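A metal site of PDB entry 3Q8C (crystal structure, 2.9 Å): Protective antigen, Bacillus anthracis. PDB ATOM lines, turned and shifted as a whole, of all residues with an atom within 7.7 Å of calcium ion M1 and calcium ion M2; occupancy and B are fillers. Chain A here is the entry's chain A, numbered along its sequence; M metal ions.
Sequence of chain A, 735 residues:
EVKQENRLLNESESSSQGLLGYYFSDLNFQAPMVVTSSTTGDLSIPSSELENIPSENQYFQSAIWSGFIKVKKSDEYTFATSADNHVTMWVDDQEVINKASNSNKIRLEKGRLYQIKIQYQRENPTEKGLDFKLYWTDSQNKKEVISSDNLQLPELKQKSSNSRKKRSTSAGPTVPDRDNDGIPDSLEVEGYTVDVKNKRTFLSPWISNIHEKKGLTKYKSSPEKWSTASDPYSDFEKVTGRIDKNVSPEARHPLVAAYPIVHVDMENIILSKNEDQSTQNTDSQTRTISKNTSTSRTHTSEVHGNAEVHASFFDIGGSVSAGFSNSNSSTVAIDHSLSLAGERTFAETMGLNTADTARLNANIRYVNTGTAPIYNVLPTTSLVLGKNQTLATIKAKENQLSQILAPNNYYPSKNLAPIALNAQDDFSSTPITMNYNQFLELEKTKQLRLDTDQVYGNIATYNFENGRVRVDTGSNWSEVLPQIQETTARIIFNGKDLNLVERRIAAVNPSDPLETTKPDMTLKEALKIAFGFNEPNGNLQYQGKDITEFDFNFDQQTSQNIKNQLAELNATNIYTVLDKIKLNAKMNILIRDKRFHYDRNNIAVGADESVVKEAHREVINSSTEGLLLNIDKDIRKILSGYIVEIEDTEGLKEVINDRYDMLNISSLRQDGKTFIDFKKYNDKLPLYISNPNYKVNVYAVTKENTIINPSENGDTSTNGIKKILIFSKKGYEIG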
ATOM      1  N   PRO A 176       5.616 -13.985 -26.859  1.00  0.00           N
ATOM      2  CA  PRO A 176       5.842 -12.530 -26.847  1.00  0.00           C
ATOM      3  C   PRO A 176       7.286 -12.128 -27.154  1.00  0.00           C
ATOM      4  O   PRO A 176       8.239 -12.555 -26.499  1.00  0.00           O
ATOM      5  CB  PRO A 176       5.443 -12.118 -25.420  1.00  0.00           C
ATOM      6  CG  PRO A 176       4.595 -13.254 -24.911  1.00  0.00           C
ATOM      7  CD  PRO A 176       5.160 -14.486 -25.554  1.00  0.00           C
ATOM      8  N   ASP A 177       7.413 -11.301 -28.180  1.00  0.00           N
ATOM      9  CA  ASP A 177       8.703 -10.891 -28.707  1.00  0.00           C
ATOM     10  C   ASP A 177       8.489  -9.504 -29.278  1.00  0.00           C
ATOM     11  O   ASP A 177       8.458  -9.312 -30.503  1.00  0.00           O
ATOM     12  CB  ASP A 177       9.141 -11.891 -29.785  1.00  0.00           C
ATOM     13  CG  ASP A 177      10.539 -11.642 -30.285  1.00  0.00           C
ATOM     14  OD1 ASP A 177      11.287 -10.886 -29.655  1.00  0.00           O
ATOM     15  OD2 ASP A 177      10.904 -12.214 -31.329  1.00  0.00           O
ATOM     16  N   ARG A 178       8.317  -8.525 -28.390  1.00  0.00           N
ATOM     17  CA  ARG A 178       7.856  -7.197 -28.771  1.00  0.00           C
ATOM     18  C   ARG A 178       8.712  -6.504 -29.805  1.00  0.00           C
ATOM     19  O   ARG A 178       8.197  -5.862 -30.707  1.00  0.00           O
ATOM     20  CB  ARG A 178       7.770  -6.288 -27.543  1.00  0.00           C
ATOM     21  CG  ARG A 178       6.647  -6.639 -26.595  1.00  0.00           C
ATOM     22  CD  ARG A 178       6.909  -6.033 -25.235  1.00  0.00           C
ATOM     23  NE  ARG A 178       5.722  -5.379 -24.696  1.00  0.00           N
ATOM     24  CZ  ARG A 178       4.593  -6.008 -24.390  1.00  0.00           C
ATOM     25  NH1 ARG A 178       4.482  -7.325 -24.559  1.00  0.00           N
ATOM     26  NH2 ARG A 178       3.566  -5.316 -23.900  1.00  0.00           N
ATOM     27  N   ASP A 179      10.028  -6.600 -29.664  1.00  0.00           N
ATOM     28  CA  ASP A 179      10.931  -5.912 -30.578  1.00  0.00           C
ATOM     29  C   ASP A 179      11.223  -6.778 -31.787  1.00  0.00           C
ATOM     30  O   ASP A 179      11.739  -6.295 -32.795  1.00  0.00           O
ATOM     31  CB  ASP A 179      12.239  -5.539 -29.879  1.00  0.00           C
ATOM     32  CG  ASP A 179      12.927  -6.722 -29.226  1.00  0.00           C
ATOM     33  OD1 ASP A 179      12.620  -7.868 -29.592  1.00  0.00           O
ATOM     34  OD2 ASP A 179      13.771  -6.507 -28.353  1.00  0.00           O
ATOM     35  N   ASN A 180      10.912  -8.068 -31.674  1.00  0.00           N
ATOM     36  CA  ASN A 180      11.068  -8.993 -32.791  1.00  0.00           C
ATOM     37  C   ASN A 180      12.544  -9.280 -33.116  1.00  0.00           C
ATOM     38  O   ASN A 180      12.920  -9.412 -34.287  1.00  0.00           O
ATOM     39  CB  ASN A 180      10.355  -8.456 -34.028  1.00  0.00           C
ATOM     40  CG  ASN A 180      10.152  -9.508 -35.085  1.00  0.00           C
ATOM     41  OD1 ASN A 180       9.784 -10.645 -34.783  1.00  0.00           O
ATOM     42  ND2 ASN A 180      10.397  -9.147 -36.336  1.00  0.00           N
ATOM     43  N   ASP A 181      13.375  -9.373 -32.079  1.00  0.00           N
ATOM     44  CA  ASP A 181      14.764  -9.783 -32.279  1.00  0.00           C
ATOM     45  C   ASP A 181      14.866 -11.300 -32.174  1.00  0.00           C
ATOM     46  O   ASP A 181      15.835 -11.886 -32.648  1.00  0.00           O
ATOM     47  CB  ASP A 181      15.720  -9.104 -31.293  1.00  0.00           C
ATOM     48  CG  ASP A 181      15.244  -9.146 -29.843  1.00  0.00           C
ATOM     49  OD1 ASP A 181      14.347  -9.934 -29.473  1.00  0.00           O
ATOM     50  OD2 ASP A 181      15.793  -8.373 -29.060  1.00  0.00           O
ATOM     51  N   GLY A 182      13.852 -11.910 -31.569  1.00  0.00           N
ATOM     52  CA  GLY A 182      13.785 -13.356 -31.449  1.00  0.00           C
ATOM     53  C   GLY A 182      13.800 -13.823 -30.003  1.00  0.00           C
ATOM     54  O   GLY A 182      13.103 -14.767 -29.652  1.00  0.00           O
ATOM     55  N   ILE A 183      14.617 -13.173 -29.178  1.00  0.00           N
ATOM     56  CA  ILE A 183      14.659 -13.468 -27.757  1.00  0.00           C
ATOM     57  C   ILE A 183      13.336 -13.053 -27.132  1.00  0.00           C
ATOM     58  O   ILE A 183      12.988 -11.880 -27.187  1.00  0.00           O
ATOM     59  CB  ILE A 183      15.779 -12.703 -27.034  1.00  0.00           C
ATOM     60  CG1 ILE A 183      17.141 -13.023 -27.639  1.00  0.00           C
ATOM     61  CG2 ILE A 183      15.803 -13.045 -25.555  1.00  0.00           C
ATOM     62  CD1 ILE A 183      18.251 -12.127 -27.144  1.00  0.00           C
ATOM     63  N   PRO A 184      12.588 -14.020 -26.547  1.00  0.00           N
ATOM     64  CA  PRO A 184      11.310 -13.692 -25.889  1.00  0.00           C
ATOM     65  C   PRO A 184      11.478 -12.599 -24.827  1.00  0.00           C
ATOM     66  O   PRO A 184      12.604 -12.369 -24.396  1.00  0.00           O
ATOM     67  CB  PRO A 184      10.891 -15.018 -25.252  1.00  0.00           C
ATOM     68  CG  PRO A 184      11.564 -16.063 -26.048  1.00  0.00           C
ATOM     69  CD  PRO A 184      12.881 -15.461 -26.459  1.00  0.00           C
ATOM     70  N   ASP A 185      10.388 -11.954 -24.433  1.00  0.00           N
ATOM     71  CA  ASP A 185      10.432 -10.838 -23.494  1.00  0.00           C
ATOM     72  C   ASP A 185      10.900 -11.267 -22.104  1.00  0.00           C
ATOM     73  O   ASP A 185      11.801 -10.665 -21.528  1.00  0.00           O
ATOM     74  CB  ASP A 185       9.062 -10.183 -23.388  1.00  0.00           C
ATOM     75  CG  ASP A 185       8.608  -9.571 -24.701  1.00  0.00           C
ATOM     76  OD1 ASP A 185       9.464  -9.368 -25.605  1.00  0.00           O
ATOM     77  OD2 ASP A 185       7.394  -9.284 -24.831  1.00  0.00           O
ATOM     78  N   SER A 186      10.288 -12.319 -21.575  1.00  0.00           N
ATOM     79  CA  SER A 186      10.609 -12.757 -20.225  1.00  0.00           C
ATOM     80  C   SER A 186      12.096 -13.032 -20.082  1.00  0.00           C
ATOM     81  O   SER A 186      12.697 -12.629 -19.087  1.00  0.00           O
ATOM     82  CB  SER A 186       9.785 -13.991 -19.846  1.00  0.00           C
ATOM     83  OG  SER A 186       9.907 -15.028 -20.804  1.00  0.00           O
ATOM     84  N   GLU A 188      14.635 -11.771 -21.768  1.00  0.00           N
ATOM     85  CA  GLU A 188      15.488 -10.601 -21.892  1.00  0.00           C
ATOM     86  C   GLU A 188      15.564  -9.847 -20.572  1.00  0.00           C
ATOM     87  O   GLU A 188      16.538  -9.149 -20.310  1.00  0.00           O
ATOM     88  CB  GLU A 188      14.963  -9.668 -22.972  1.00  0.00           C
ATOM     89  CG  GLU A 188      15.049 -10.239 -24.369  1.00  0.00           C
ATOM     90  CD  GLU A 188      15.217  -9.160 -25.422  1.00  0.00           C
ATOM     91  OE1 GLU A 188      14.488  -9.165 -26.439  1.00  0.00           O
ATOM     92  OE2 GLU A 188      16.118  -8.314 -25.234  1.00  0.00           O
ATOM     93  N   TYR A 192      19.718 -14.305 -19.245  1.00  0.00           N
ATOM     94  CA  TYR A 192      19.885 -15.499 -20.064  1.00  0.00           C
ATOM     95  C   TYR A 192      21.356 -15.700 -20.406  1.00  0.00           C
ATOM     96  O   TYR A 192      22.146 -14.764 -20.332  1.00  0.00           O
ATOM     97  CB  TYR A 192      19.042 -15.402 -21.343  1.00  0.00           C
ATOM     98  CG  TYR A 192      19.367 -14.215 -22.228  1.00  0.00           C
ATOM     99  CD1 TYR A 192      18.826 -12.966 -21.959  1.00  0.00           C
ATOM    100  CD2 TYR A 192      20.221 -14.342 -23.326  1.00  0.00           C
ATOM    101  CE1 TYR A 192      19.122 -11.878 -22.750  1.00  0.00           C
ATOM    102  CE2 TYR A 192      20.532 -13.260 -24.112  1.00  0.00           C
ATOM    103  CZ  TYR A 192      19.972 -12.031 -23.825  1.00  0.00           C
ATOM    104  OH  TYR A 192      20.268 -10.934 -24.606  1.00  0.00           O
ATOM    105  N   LYS A 220      21.418  -9.523 -19.995  1.00  0.00           N
ATOM    106  CA  LYS A 220      20.137  -8.847 -19.901  1.00  0.00           C
ATOM    107  C   LYS A 220      20.022  -7.815 -21.029  1.00  0.00           C
ATOM    108  O   LYS A 220      21.038  -7.317 -21.532  1.00  0.00           O
ATOM    109  CB  LYS A 220      19.960  -8.192 -18.541  1.00  0.00           C
ATOM    110  CG  LYS A 220      19.466  -9.137 -17.463  1.00  0.00           C
ATOM    111  CD  LYS A 220      19.565  -8.502 -16.082  1.00  0.00           C
ATOM    112  CE  LYS A 220      18.947  -9.391 -15.008  1.00  0.00           C
ATOM    113  NZ  LYS A 220      19.135  -8.844 -13.632  1.00  0.00           N
ATOM    114  N   SER A 221      18.794  -7.501 -21.410  1.00  0.00           N
ATOM    115  CA  SER A 221      18.554  -6.584 -22.537  1.00  0.00           C
ATOM    116  C   SER A 221      17.084  -6.153 -22.626  1.00  0.00           C
ATOM    117  O   SER A 221      16.205  -6.761 -22.020  1.00  0.00           O
ATOM    118  CB  SER A 221      19.018  -7.229 -23.848  1.00  0.00           C
ATOM    119  OG  SER A 221      18.514  -8.551 -23.983  1.00  0.00           O
ATOM    120  N   SER A 222      16.831  -5.088 -23.388  1.00  0.00           N
ATOM    121  CA  SER A 222      15.488  -4.496 -23.488  1.00  0.00           C
ATOM    122  C   SER A 222      14.560  -5.309 -24.384  1.00  0.00           C
ATOM    123  O   SER A 222      14.852  -5.512 -25.546  1.00  0.00           O
ATOM    124  CB  SER A 222      15.577  -3.070 -24.025  1.00  0.00           C
ATOM    125  OG  SER A 222      14.291  -2.563 -24.333  1.00  0.00           O
ATOM    126  N   PRO A 223      13.425  -5.756 -23.843  1.00  0.00           N
ATOM    127  CA  PRO A 223      12.510  -6.516 -24.710  1.00  0.00           C
ATOM    128  C   PRO A 223      11.772  -5.614 -25.698  1.00  0.00           C
ATOM    129  O   PRO A 223      10.976  -6.113 -26.493  1.00  0.00           O
ATOM    130  CB  PRO A 223      11.523  -7.149 -23.719  1.00  0.00           C
ATOM    131  CG  PRO A 223      11.576  -6.257 -22.502  1.00  0.00           C
ATOM    132  CD  PRO A 223      12.962  -5.678 -22.448  1.00  0.00           C
ATOM    133  N   GLU A 224      12.039  -4.303 -25.632  1.00  0.00           N
ATOM    134  CA  GLU A 224      11.393  -3.299 -26.480  1.00  0.00           C
ATOM    135  C   GLU A 224      12.370  -2.688 -27.489  1.00  0.00           C
ATOM    136  O   GLU A 224      11.973  -1.898 -28.345  1.00  0.00           O
ATOM    137  CB  GLU A 224      10.800  -2.174 -25.626  1.00  0.00           C
ATOM    138  CG  GLU A 224      10.345  -2.597 -24.211  1.00  0.00           C
ATOM    139  CD  GLU A 224       8.908  -3.115 -24.157  1.00  0.00           C
ATOM    140  OE1 GLU A 224       8.602  -3.890 -23.221  1.00  0.00           O
ATOM    141  OE2 GLU A 224       8.084  -2.728 -25.024  1.00  0.00           O
ATOM    142  N   LYS A 225      13.638  -3.049 -27.383  1.00  0.00           N
ATOM    143  CA  LYS A 225      14.635  -2.589 -28.342  1.00  0.00           C
ATOM    144  C   LYS A 225      15.190  -3.767 -29.139  1.00  0.00           C
ATOM    145  O   LYS A 225      15.878  -4.622 -28.603  1.00  0.00           O
ATOM    146  CB  LYS A 225      15.755  -1.855 -27.620  1.00  0.00           C
ATOM    147  CG  LYS A 225      15.240  -0.846 -26.619  1.00  0.00           C
ATOM    148  CD  LYS A 225      16.302   0.149 -26.241  1.00  0.00           C
ATOM    149  CE  LYS A 225      16.447   1.163 -27.330  1.00  0.00           C
ATOM    150  NZ  LYS A 225      17.830   1.596 -27.495  1.00  0.00           N
ATOM    151  N   TRP A 226      14.886  -3.813 -30.429  1.00  0.00           N
ATOM    152  CA  TRP A 226      15.452  -4.827 -31.300  1.00  0.00           C
ATOM    153  C   TRP A 226      16.951  -4.918 -31.026  1.00  0.00           C
ATOM    154  O   TRP A 226      17.525  -6.005 -30.916  1.00  0.00           O
ATOM    155  CB  TRP A 226      15.211  -4.453 -32.748  1.00  0.00           C
ATOM    156  CG  TRP A 226      15.755  -5.447 -33.717  1.00  0.00           C
ATOM    157  CD1 TRP A 226      15.256  -6.672 -33.980  1.00  0.00           C
ATOM    158  CD2 TRP A 226      16.896  -5.287 -34.572  1.00  0.00           C
ATOM    159  NE1 TRP A 226      16.014  -7.300 -34.942  1.00  0.00           N
ATOM    160  CE2 TRP A 226      17.027  -6.472 -35.324  1.00  0.00           C
ATOM    161  CE3 TRP A 226      17.831  -4.250 -34.765  1.00  0.00           C
ATOM    162  CZ2 TRP A 226      18.043  -6.658 -36.261  1.00  0.00           C
ATOM    163  CZ3 TRP A 226      18.838  -4.439 -35.699  1.00  0.00           C
ATOM    164  CH2 TRP A 226      18.943  -5.634 -36.441  1.00  0.00           C
ATOM    165  N   SER A 227      17.575  -3.750 -30.943  1.00  0.00           N
ATOM    166  CA  SER A 227      18.962  -3.655 -30.533  1.00  0.00           C
ATOM    167  C   SER A 227      19.047  -2.732 -29.317  1.00  0.00           C
ATOM    168  O   SER A 227      18.671  -1.564 -29.394  1.00  0.00           O
ATOM    169  CB  SER A 227      19.826  -3.144 -31.674  1.00  0.00           C
ATOM    170  OG  SER A 227      21.021  -2.570 -31.192  1.00  0.00           O
ATOM    171  N   THR A 228      19.544  -3.265 -28.200  1.00  0.00           N
ATOM    172  CA  THR A 228      19.471  -2.574 -26.921  1.00  0.00           C
ATOM    173  C   THR A 228      20.479  -1.440 -26.784  1.00  0.00           C
ATOM    174  O   THR A 228      20.281  -0.517 -25.995  1.00  0.00           O
ATOM    175  CB  THR A 228      19.648  -3.550 -25.750  1.00  0.00           C
ATOM    176  OG1 THR A 228      18.455  -4.332 -25.619  1.00  0.00           O
ATOM    177  CG2 THR A 228      19.918  -2.802 -24.463  1.00  0.00           C
ATOM    178  N   SER A 234      21.081  -6.956 -33.898  1.00  0.00           N
ATOM    179  CA  SER A 234      20.055  -7.255 -32.879  1.00  0.00           C
ATOM    180  C   SER A 234      20.614  -7.948 -31.642  1.00  0.00           C
ATOM    181  O   SER A 234      21.730  -8.441 -31.622  1.00  0.00           O
ATOM    182  CB  SER A 234      18.914  -8.080 -33.478  1.00  0.00           C
ATOM    183  OG  SER A 234      19.350  -9.362 -33.879  1.00  0.00           O
ATOM    184  N   ASP A 235      19.817  -7.977 -30.583  1.00  0.00           N
ATOM    185  CA  ASP A 235      20.291  -8.548 -29.351  1.00  0.00           C
ATOM    186  C   ASP A 235      20.412 -10.055 -29.521  1.00  0.00           C
ATOM    187  O   ASP A 235      21.150 -10.725 -28.782  1.00  0.00           O
ATOM    188  CB  ASP A 235      19.361  -8.145 -28.202  1.00  0.00           C
ATOM    189  CG  ASP A 235      19.345  -6.641 -27.997  1.00  0.00           C
ATOM    190  OD1 ASP A 235      20.410  -5.989 -28.180  1.00  0.00           O
ATOM    191  OD2 ASP A 235      18.285  -6.090 -27.683  1.00  0.00           O
ATOM    192  N   PHE A 236      19.712 -10.573 -30.536  1.00  0.00           N
ATOM    193  CA  PHE A 236      19.743 -11.999 -30.862  1.00  0.00           C
ATOM    194  C   PHE A 236      20.867 -12.302 -31.846  1.00  0.00           C
ATOM    195  O   PHE A 236      21.485 -13.355 -31.794  1.00  0.00           O
ATOM    196  CB  PHE A 236      18.397 -12.411 -31.462  1.00  0.00           C
ATOM    197  CG  PHE A 236      18.297 -13.852 -31.822  1.00  0.00           C
ATOM    198  CD1 PHE A 236      18.065 -14.812 -30.847  1.00  0.00           C
ATOM    199  CD2 PHE A 236      18.370 -14.260 -33.144  1.00  0.00           C
ATOM    200  CE1 PHE A 236      17.947 -16.156 -31.187  1.00  0.00           C
ATOM    201  CE2 PHE A 236      18.248 -15.604 -33.493  1.00  0.00           C
ATOM    202  CZ  PHE A 236      18.031 -16.547 -32.523  1.00  0.00           C
ATOM    203  N   PRO A 254      24.847  -7.570 -25.734  1.00  0.00           N
ATOM    204  CA  PRO A 254      23.667  -6.748 -26.071  1.00  0.00           C
ATOM    205  C   PRO A 254      23.764  -5.310 -25.569  1.00  0.00           C
ATOM    206  O   PRO A 254      23.078  -4.433 -26.106  1.00  0.00           O
ATOM    207  CB  PRO A 254      22.535  -7.469 -25.349  1.00  0.00           C
ATOM    208  CG  PRO A 254      22.957  -8.890 -25.321  1.00  0.00           C
ATOM    209  CD  PRO A 254      24.458  -8.883 -25.184  1.00  0.00           C
HETATM  210 CA    CA M   1      15.931  -6.857 -27.273  1.00  0.00          CA
HETATM  211 CA    CA M   2      12.296  -9.430 -27.724  1.00  0.00          CA
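The backbone NH (N) of Ser 222 is in hydrogen-bond range of the side-chain hydroxyl (OG1) of Thr 228 (2.9 Å). N of Glu 224 sits close to OG of Ser 222. N of Thr 228 lies within hydrogen-bond range of OD1 of Asp 235 (2.9 Å). The backbone NH (N) of Asp 235 sits at hydrogen-bond distance from the backbone carbonyl oxygen (O) of Trp 226. The backbone carbonyl oxygen (O) of Glu 188 sits at hydrogen-bond distance from the backbone NH (N) of Ser 221, at 3.0 Å. The side-chain carboxylate (OD2) of Asp 177 lies within hydrogen-bond range of the backbone NH (N) of Gly 182, 3.0 Å away. OD2 of Asp 185 is in salt-bridge range of NH1 of Arg 178 (3.5 Å). The backbone carbonyl oxygen (O) of Pro 176 lies within hydrogen-bond range of the backbone NH (N) of Asp 185 (3.0 Å).
Merely in contact with calcium ion M1: Thr 228 (3.9 Å). Along chain A the residues within 4 Å of calcium ion M1 span positions 179 to 235. The nearest printed residue that does not touch calcium ion M1 is Trp 226 (4.1 Å).
Merely in contact with calcium ion M2: Asp 185 and Pro 223. Within 4 Å of calcium ion M2: Asp 177, Asp 179, Asp 181, Ile 183, Asp 185, Glu 188 and Pro 223. The nearest printed residue that does not touch calcium ion M2 is Arg 178 (4.1 Å).
Calcium ion M1 is bound by the side-chain carboxylate (OD2) of Asp 181 (2.3 Å), the backbone carbonyl oxygen (O) of Ser 222 (2.4 Å), the side-chain carboxylate (OD2) of Asp 179 (2.4 Å), the side-chain carboxylate (OD2) of Asp 235 (2.5 Å), the side-chain carboxylate (OE2) of Glu 188 (2.5 Å), the backbone carbonyl oxygen (O) of Lys 225 (2.6 Å) and the side-chain carboxylate (OE1) of Glu 188 (2.8 Å).
Calcium ion M2 is bound by OD1 of Asp 179 (2.5 Å), OE1 of Glu 188 (2.6 Å), O of Ile 183 (2.6 Å), OD1 of Asp 177 (2.6 Å) and OD1 of Asp 181 (2.7 Å).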
